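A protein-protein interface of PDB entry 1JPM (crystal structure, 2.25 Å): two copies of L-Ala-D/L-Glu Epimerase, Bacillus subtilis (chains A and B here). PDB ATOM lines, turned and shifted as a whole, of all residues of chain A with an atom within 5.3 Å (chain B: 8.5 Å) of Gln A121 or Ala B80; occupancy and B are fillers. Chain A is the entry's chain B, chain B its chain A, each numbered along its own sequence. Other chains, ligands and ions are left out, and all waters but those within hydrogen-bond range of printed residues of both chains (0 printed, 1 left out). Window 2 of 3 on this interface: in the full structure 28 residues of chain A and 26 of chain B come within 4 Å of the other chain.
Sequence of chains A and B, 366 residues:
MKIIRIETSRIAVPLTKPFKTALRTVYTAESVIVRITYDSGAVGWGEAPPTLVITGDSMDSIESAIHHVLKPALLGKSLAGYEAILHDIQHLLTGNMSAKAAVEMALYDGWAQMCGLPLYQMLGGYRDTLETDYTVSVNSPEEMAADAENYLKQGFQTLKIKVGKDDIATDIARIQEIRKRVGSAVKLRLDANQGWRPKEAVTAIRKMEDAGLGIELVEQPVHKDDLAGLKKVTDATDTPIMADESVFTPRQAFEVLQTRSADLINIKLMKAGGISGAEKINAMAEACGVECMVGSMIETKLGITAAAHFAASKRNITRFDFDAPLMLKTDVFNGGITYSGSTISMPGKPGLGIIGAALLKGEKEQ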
ATOM      1  N   LEU A 117       6.135  26.774  -9.211  1.00  0.00           N
ATOM      2  CA  LEU A 117       7.173  26.005  -9.889  1.00  0.00           C
ATOM      3  C   LEU A 117       7.306  26.334 -11.370  1.00  0.00           C
ATOM      4  O   LEU A 117       6.361  26.815 -12.000  1.00  0.00           O
ATOM      5  CB  LEU A 117       6.877  24.507  -9.781  1.00  0.00           C
ATOM      6  CG  LEU A 117       6.841  23.805  -8.424  1.00  0.00           C
ATOM      7  CD1 LEU A 117       6.201  22.434  -8.602  1.00  0.00           C
ATOM      8  CD2 LEU A 117       8.254  23.682  -7.856  1.00  0.00           C
ATOM      9  N   PRO A 118       8.502  26.102 -11.939  1.00  0.00           N
ATOM     10  CA  PRO A 118       8.710  26.363 -13.367  1.00  0.00           C
ATOM     11  C   PRO A 118       7.790  25.315 -14.001  1.00  0.00           C
ATOM     12  O   PRO A 118       7.679  24.217 -13.465  1.00  0.00           O
ATOM     13  CB  PRO A 118      10.183  26.014 -13.570  1.00  0.00           C
ATOM     14  CG  PRO A 118      10.792  26.345 -12.262  1.00  0.00           C
ATOM     15  CD  PRO A 118       9.783  25.820 -11.266  1.00  0.00           C
ATOM     16  N   LEU A 119       7.136  25.631 -15.111  1.00  0.00           N
ATOM     17  CA  LEU A 119       6.222  24.675 -15.733  1.00  0.00           C
ATOM     18  C   LEU A 119       6.817  23.286 -15.966  1.00  0.00           C
ATOM     19  O   LEU A 119       6.158  22.276 -15.706  1.00  0.00           O
ATOM     20  CB  LEU A 119       5.687  25.223 -17.059  1.00  0.00           C
ATOM     21  CG  LEU A 119       4.730  24.276 -17.798  1.00  0.00           C
ATOM     22  CD1 LEU A 119       3.518  23.969 -16.916  1.00  0.00           C
ATOM     23  CD2 LEU A 119       4.281  24.914 -19.110  1.00  0.00           C
ATOM     24  N   TYR A 120       8.062  23.233 -16.439  1.00  0.00           N
ATOM     25  CA  TYR A 120       8.704  21.956 -16.713  1.00  0.00           C
ATOM     26  C   TYR A 120       8.843  21.083 -15.467  1.00  0.00           C
ATOM     27  O   TYR A 120       8.818  19.855 -15.565  1.00  0.00           O
ATOM     28  CB  TYR A 120      10.071  22.178 -17.378  1.00  0.00           C
ATOM     29  CG  TYR A 120      11.236  22.437 -16.446  1.00  0.00           C
ATOM     30  CD1 TYR A 120      12.078  21.396 -16.046  1.00  0.00           C
ATOM     31  CD2 TYR A 120      11.521  23.725 -15.991  1.00  0.00           C
ATOM     32  CE1 TYR A 120      13.179  21.630 -15.221  1.00  0.00           C
ATOM     33  CE2 TYR A 120      12.618  23.971 -15.165  1.00  0.00           C
ATOM     34  CZ  TYR A 120      13.443  22.921 -14.785  1.00  0.00           C
ATOM     35  OH  TYR A 120      14.539  23.155 -13.977  1.00  0.00           O
ATOM     36  N   GLN A 121       8.977  21.704 -14.298  1.00  0.00           N
ATOM     37  CA  GLN A 121       9.102  20.927 -13.067  1.00  0.00           C
ATOM     38  C   GLN A 121       7.722  20.448 -12.637  1.00  0.00           C
ATOM     39  O   GLN A 121       7.570  19.343 -12.107  1.00  0.00           O
ATOM     40  CB  GLN A 121       9.761  21.755 -11.958  1.00  0.00           C
ATOM     41  CG  GLN A 121      11.274  21.836 -12.085  1.00  0.00           C
ATOM     42  CD  GLN A 121      11.914  22.654 -10.980  1.00  0.00           C
ATOM     43  OE1 GLN A 121      11.231  23.132 -10.070  1.00  0.00           O
ATOM     44  NE2 GLN A 121      13.232  22.823 -11.054  1.00  0.00           N
ATOM     45  N   MET A 122       6.721  21.284 -12.881  1.00  0.00           N
ATOM     46  CA  MET A 122       5.352  20.935 -12.553  1.00  0.00           C
ATOM     47  C   MET A 122       4.911  19.733 -13.387  1.00  0.00           C
ATOM     48  O   MET A 122       4.128  18.913 -12.934  1.00  0.00           O
ATOM     49  CB  MET A 122       4.415  22.134 -12.792  1.00  0.00           C
ATOM     50  CG  MET A 122       2.947  21.770 -12.828  1.00  0.00           C
ATOM     51  SD  MET A 122       1.880  23.141 -12.538  1.00  0.00           S
ATOM     52  CE  MET A 122       2.287  23.295 -10.832  1.00  0.00           C
ATOM     53  N   LEU A 123       5.453  19.605 -14.593  1.00  0.00           N
ATOM     54  CA  LEU A 123       5.086  18.495 -15.456  1.00  0.00           C
ATOM     55  C   LEU A 123       5.959  17.247 -15.315  1.00  0.00           C
ATOM     56  O   LEU A 123       5.691  16.224 -15.956  1.00  0.00           O
ATOM     57  CB  LEU A 123       5.072  18.972 -16.909  1.00  0.00           C
ATOM     58  CG  LEU A 123       4.064  20.080 -17.205  1.00  0.00           C
ATOM     59  CD1 LEU A 123       4.252  20.549 -18.628  1.00  0.00           C
ATOM     60  CD2 LEU A 123       2.652  19.568 -16.969  1.00  0.00           C
ATOM     61  N   GLY A 124       6.993  17.312 -14.477  1.00  0.00           N
ATOM     62  CA  GLY A 124       7.844  16.144 -14.302  1.00  0.00           C
ATOM     63  C   GLY A 124       9.314  16.447 -14.085  1.00  0.00           C
ATOM     64  O   GLY A 124      10.046  15.621 -13.544  1.00  0.00           O
ATOM     65  N   GLY A 125       9.736  17.627 -14.531  1.00  0.00           N
ATOM     66  CA  GLY A 125      11.110  18.073 -14.373  1.00  0.00           C
ATOM     67  C   GLY A 125      12.225  17.107 -14.726  1.00  0.00           C
ATOM     68  O   GLY A 125      13.254  17.093 -14.049  1.00  0.00           O
ATOM     69  N   SER A 313      10.151  18.294 -19.453  1.00  0.00           N
ATOM     70  CA  SER A 313       9.546  17.565 -18.344  1.00  0.00           C
ATOM     71  C   SER A 313       9.401  16.057 -18.483  1.00  0.00           C
ATOM     72  O   SER A 313       9.247  15.372 -17.472  1.00  0.00           O
ATOM     73  CB  SER A 313       8.157  18.136 -18.041  1.00  0.00           C
ATOM     74  OG  SER A 313       7.211  17.654 -18.974  1.00  0.00           O
ATOM     75  N   MET B   1      11.236  20.355  -2.238  1.00  0.00           N
ATOM     76  CA  MET B   1      10.926  19.440  -1.110  1.00  0.00           C
ATOM     77  C   MET B   1      11.642  18.121  -1.373  1.00  0.00           C
ATOM     78  O   MET B   1      11.456  17.523  -2.427  1.00  0.00           O
ATOM     79  CB  MET B   1       9.416  19.226  -1.047  1.00  0.00           C
ATOM     80  CG  MET B   1       8.900  18.752   0.286  1.00  0.00           C
ATOM     81  SD  MET B   1       7.158  19.140   0.424  1.00  0.00           S
ATOM     82  CE  MET B   1       6.410  17.531   0.350  1.00  0.00           C
ATOM     83  N   LYS B   2      12.466  17.678  -0.425  1.00  0.00           N
ATOM     84  CA  LYS B   2      13.212  16.432  -0.577  1.00  0.00           C
ATOM     85  C   LYS B   2      12.791  15.379   0.429  1.00  0.00           C
ATOM     86  O   LYS B   2      12.427  15.690   1.564  1.00  0.00           O
ATOM     87  CB  LYS B   2      14.717  16.665  -0.404  1.00  0.00           C
ATOM     88  CG  LYS B   2      15.351  17.619  -1.402  1.00  0.00           C
ATOM     89  CD  LYS B   2      16.822  17.853  -1.066  1.00  0.00           C
ATOM     90  CE  LYS B   2      17.429  18.959  -1.928  1.00  0.00           C
ATOM     91  NZ  LYS B   2      18.822  19.318  -1.511  1.00  0.00           N
ATOM     92  N   ILE B   3      12.869  14.123   0.005  1.00  0.00           N
ATOM     93  CA  ILE B   3      12.534  12.994   0.859  1.00  0.00           C
ATOM     94  C   ILE B   3      13.724  12.774   1.790  1.00  0.00           C
ATOM     95  O   ILE B   3      14.863  12.690   1.329  1.00  0.00           O
ATOM     96  CB  ILE B   3      12.321  11.726   0.018  1.00  0.00           C
ATOM     97  CG1 ILE B   3      11.116  11.911  -0.904  1.00  0.00           C
ATOM     98  CG2 ILE B   3      12.163  10.523   0.928  1.00  0.00           C
ATOM     99  CD1 ILE B   3      10.980  10.819  -1.949  1.00  0.00           C
ATOM    100  N   LYS B  77      16.032  12.405  -2.839  1.00  0.00           N
ATOM    101  CA  LYS B  77      15.455  12.892  -4.092  1.00  0.00           C
ATOM    102  C   LYS B  77      14.491  14.065  -3.888  1.00  0.00           C
ATOM    103  O   LYS B  77      13.777  14.142  -2.882  1.00  0.00           O
ATOM    104  CB  LYS B  77      14.728  11.756  -4.829  1.00  0.00           C
ATOM    105  CG  LYS B  77      15.640  10.633  -5.327  1.00  0.00           C
ATOM    106  CD  LYS B  77      16.704  11.147  -6.298  1.00  0.00           C
ATOM    107  CE  LYS B  77      17.562  10.004  -6.837  1.00  0.00           C
ATOM    108  NZ  LYS B  77      18.186   9.199  -5.750  1.00  0.00           N
ATOM    109  N   SER B  78      14.476  14.969  -4.863  1.00  0.00           N
ATOM    110  CA  SER B  78      13.615  16.147  -4.839  1.00  0.00           C
ATOM    111  C   SER B  78      12.362  15.904  -5.689  1.00  0.00           C
ATOM    112  O   SER B  78      12.454  15.372  -6.795  1.00  0.00           O
ATOM    113  CB  SER B  78      14.390  17.354  -5.376  1.00  0.00           C
ATOM    114  OG  SER B  78      13.545  18.478  -5.537  1.00  0.00           O
ATOM    115  N   LEU B  79      11.197  16.287  -5.175  1.00  0.00           N
ATOM    116  CA  LEU B  79       9.947  16.093  -5.910  1.00  0.00           C
ATOM    117  C   LEU B  79       9.823  17.024  -7.112  1.00  0.00           C
ATOM    118  O   LEU B  79       8.876  16.918  -7.894  1.00  0.00           O
ATOM    119  CB  LEU B  79       8.732  16.273  -4.990  1.00  0.00           C
ATOM    120  CG  LEU B  79       8.663  15.325  -3.787  1.00  0.00           C
ATOM    121  CD1 LEU B  79       7.259  15.346  -3.204  1.00  0.00           C
ATOM    122  CD2 LEU B  79       9.024  13.916  -4.210  1.00  0.00           C
ATOM    123  N   ALA B  80      10.776  17.941  -7.251  1.00  0.00           N
ATOM    124  CA  ALA B  80      10.777  18.848  -8.387  1.00  0.00           C
ATOM    125  C   ALA B  80      11.203  18.006  -9.593  1.00  0.00           C
ATOM    126  O   ALA B  80      11.137  18.456 -10.740  1.00  0.00           O
ATOM    127  CB  ALA B  80      11.762  19.991  -8.154  1.00  0.00           C
ATOM    128  N   GLY B  81      11.646  16.782  -9.306  1.00  0.00           N
ATOM    129  CA  GLY B  81      12.063  15.843 -10.342  1.00  0.00           C
ATOM    130  C   GLY B  81      11.240  14.568 -10.196  1.00  0.00           C
ATOM    131  O   GLY B  81      11.772  13.479  -9.973  1.00  0.00           O
ATOM    132  N   TYR B  82       9.929  14.722 -10.328  1.00  0.00           N
ATOM    133  CA  TYR B  82       8.969  13.632 -10.172  1.00  0.00           C
ATOM    134  C   TYR B  82       9.079  12.509 -11.209  1.00  0.00           C
ATOM    135  O   TYR B  82       9.001  11.324 -10.873  1.00  0.00           O
ATOM    136  CB  TYR B  82       7.558  14.222 -10.195  1.00  0.00           C
ATOM    137  CG  TYR B  82       6.581  13.525  -9.287  1.00  0.00           C
ATOM    138  CD1 TYR B  82       6.805  13.455  -7.911  1.00  0.00           C
ATOM    139  CD2 TYR B  82       5.417  12.954  -9.795  1.00  0.00           C
ATOM    140  CE1 TYR B  82       5.885  12.833  -7.062  1.00  0.00           C
ATOM    141  CE2 TYR B  82       4.491  12.332  -8.958  1.00  0.00           C
ATOM    142  CZ  TYR B  82       4.732  12.275  -7.596  1.00  0.00           C
ATOM    143  OH  TYR B  82       3.818  11.655  -6.776  1.00  0.00           O
ATOM    144  N   GLU B  83       9.250  12.893 -12.467  1.00  0.00           N
ATOM    145  CA  GLU B  83       9.363  11.946 -13.570  1.00  0.00           C
ATOM    146  C   GLU B  83      10.425  10.886 -13.277  1.00  0.00           C
ATOM    147  O   GLU B  83      10.152   9.692 -13.381  1.00  0.00           O
ATOM    148  CB  GLU B  83       9.707  12.710 -14.854  1.00  0.00           C
ATOM    149  CG  GLU B  83       9.783  11.884 -16.138  1.00  0.00           C
ATOM    150  CD  GLU B  83       8.420  11.647 -16.804  1.00  0.00           C
ATOM    151  OE1 GLU B  83       8.406  11.403 -18.028  1.00  0.00           O
ATOM    152  OE2 GLU B  83       7.377  11.687 -16.117  1.00  0.00           O
ATOM    153  N   ALA B  84      11.628  11.316 -12.896  1.00  0.00           N
ATOM    154  CA  ALA B  84      12.707  10.370 -12.609  1.00  0.00           C
ATOM    155  C   ALA B  84      12.354   9.457 -11.438  1.00  0.00           C
ATOM    156  O   ALA B  84      12.673   8.270 -11.448  1.00  0.00           O
ATOM    157  CB  ALA B  84      14.014  11.121 -12.319  1.00  0.00           C
ATOM    158  N   ILE B  85      11.699  10.016 -10.425  1.00  0.00           N
ATOM    159  CA  ILE B  85      11.294   9.242  -9.259  1.00  0.00           C
ATOM    160  C   ILE B  85      10.268   8.168  -9.657  1.00  0.00           C
ATOM    161  O   ILE B  85      10.408   7.000  -9.289  1.00  0.00           O
ATOM    162  CB  ILE B  85      10.679  10.161  -8.177  1.00  0.00           C
ATOM    163  CG1 ILE B  85      11.751  11.112  -7.632  1.00  0.00           C
ATOM    164  CG2 ILE B  85      10.076   9.321  -7.054  1.00  0.00           C
ATOM    165  CD1 ILE B  85      11.211  12.167  -6.676  1.00  0.00           C
ATOM    166  N   TRP B 111       3.659  15.409  -3.011  1.00  0.00           N
ATOM    167  CA  TRP B 111       3.669  16.241  -4.206  1.00  0.00           C
ATOM    168  C   TRP B 111       2.525  17.256  -4.156  1.00  0.00           C
ATOM    169  O   TRP B 111       2.707  18.429  -4.489  1.00  0.00           O
ATOM    170  CB  TRP B 111       3.547  15.351  -5.447  1.00  0.00           C
ATOM    171  CG  TRP B 111       3.653  16.078  -6.742  1.00  0.00           C
ATOM    172  CD1 TRP B 111       4.725  16.788  -7.201  1.00  0.00           C
ATOM    173  CD2 TRP B 111       2.648  16.162  -7.757  1.00  0.00           C
ATOM    174  NE1 TRP B 111       4.447  17.313  -8.442  1.00  0.00           N
ATOM    175  CE2 TRP B 111       3.178  16.945  -8.806  1.00  0.00           C
ATOM    176  CE3 TRP B 111       1.346  15.654  -7.883  1.00  0.00           C
ATOM    177  CZ2 TRP B 111       2.453  17.233  -9.968  1.00  0.00           C
ATOM    178  CZ3 TRP B 111       0.623  15.941  -9.040  1.00  0.00           C
ATOM    179  CH2 TRP B 111       1.181  16.723 -10.067  1.00  0.00           C
ATOM    180  N   MET B 114       3.293  19.796  -1.598  1.00  0.00           N
ATOM    181  CA  MET B 114       4.330  20.707  -2.075  1.00  0.00           C
ATOM    182  C   MET B 114       3.747  21.792  -2.978  1.00  0.00           C
ATOM    183  O   MET B 114       4.289  22.900  -3.061  1.00  0.00           O
ATOM    184  CB  MET B 114       5.420  19.948  -2.844  1.00  0.00           C
ATOM    185  CG  MET B 114       6.449  20.864  -3.508  1.00  0.00           C
ATOM    186  SD  MET B 114       7.703  20.014  -4.490  1.00  0.00           S
ATOM    187  CE  MET B 114       6.780  19.678  -5.992  1.00  0.00           C
ATOM    188  N   CYS B 115       2.650  21.466  -3.659  1.00  0.00           N
ATOM    189  CA  CYS B 115       1.994  22.417  -4.551  1.00  0.00           C
ATOM    190  C   CYS B 115       0.815  23.047  -3.817  1.00  0.00           C
ATOM    191  O   CYS B 115       0.108  23.891  -4.363  1.00  0.00           O
ATOM    192  CB  CYS B 115       1.509  21.717  -5.834  1.00  0.00           C
ATOM    193  SG  CYS B 115       2.831  21.033  -6.896  1.00  0.00           S
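Leu A119 touches none of the printed residues of chain B.
Of chain B, only Ala B80 comes within 4 Å of Gln A121.
Of chain B, only Gly B81, Tyr B82 and Glu B83 come within 4 Å of Gly A124.
Gly A125 touches just one residue of chain B: Ala B80.
Of the printed residues of chain A, Ala B80 touches Gln A121 (3.6 Å) and Gly A125 (3.7 Å).
Of the printed residues of chain A, Gly B81 touches Gly A124 (3.7 Å).
Of the printed residues of chain A, Glu B83 touches Gly A124 (3.0 Å) and Ser A313 (3.8 Å).
Of the printed residues of chain A, Met B114 touches Leu A117 (3.8 Å).
Cys B115 touches none of the printed residues of chain A.
The nearest residue of chain B that does not touch Gln A121 is Leu B79 (5.0 Å).
The nearest residue of chain A that does not touch Ala B80 is Gly A124 (4.1 Å).
The nearest printed residue of chain B that does not touch Leu A117 is Cys B115 (4.03 Å).
N of Tyr B82 lies within hydrogen-bond range of O of Gly A124, at 3.3 Å.
O of Gly A124 lies within hydrogen-bond range of N of Glu B83 (3.0 Å).
No position is printed for both chains.
Of the 8 pairs that touch across the chains among the printed residues, none has its exchanged pair printed and touching as well.
Of the 10 printed residues of chain A, 6 touch a printed residue of chain B.
Hydrophobic or aromatic side chains of chain B that line the printed part of chain A: Ala B80, Trp B111 and Met B114.
Among the printed residues, 8 pairs touch across the chains.
Among the printed residues, no Asp or Glu carboxylate lies within 4 Å of a Lys or Arg side-chain nitrogen of the other chain.
The backbone NH of Ala B80 lies close to the side-chain hydroxyl of Ser B78 (3.3 Å).
O of Trp B111 is in hydrogen-bond range of SG of Cys B115 (3.5 Å).
NE2 of Gln A121 sits at hydrogen-bond distance from OH of Tyr A120 (3.2 Å).
The backbone carbonyl oxygen (O) of Tyr A120 lies within hydrogen-bond range of the backbone NH (N) of Gly A125, at 2.6 Å.
Leu A117 touches Met B114 (CD1 to CE, 3.8 Å).
O of Ala B80 touches CG of Gln A121 (3.6 Å).
Trp B111 touches Met A122 (CZ2 to O, 3.8 Å).
Gly A124 touches Gly B81.
O of Ala B80 touches CA of Gly A125, at 3.7 Å.
Ser A313 touches Glu B83 (O to CB, 3.8 Å).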
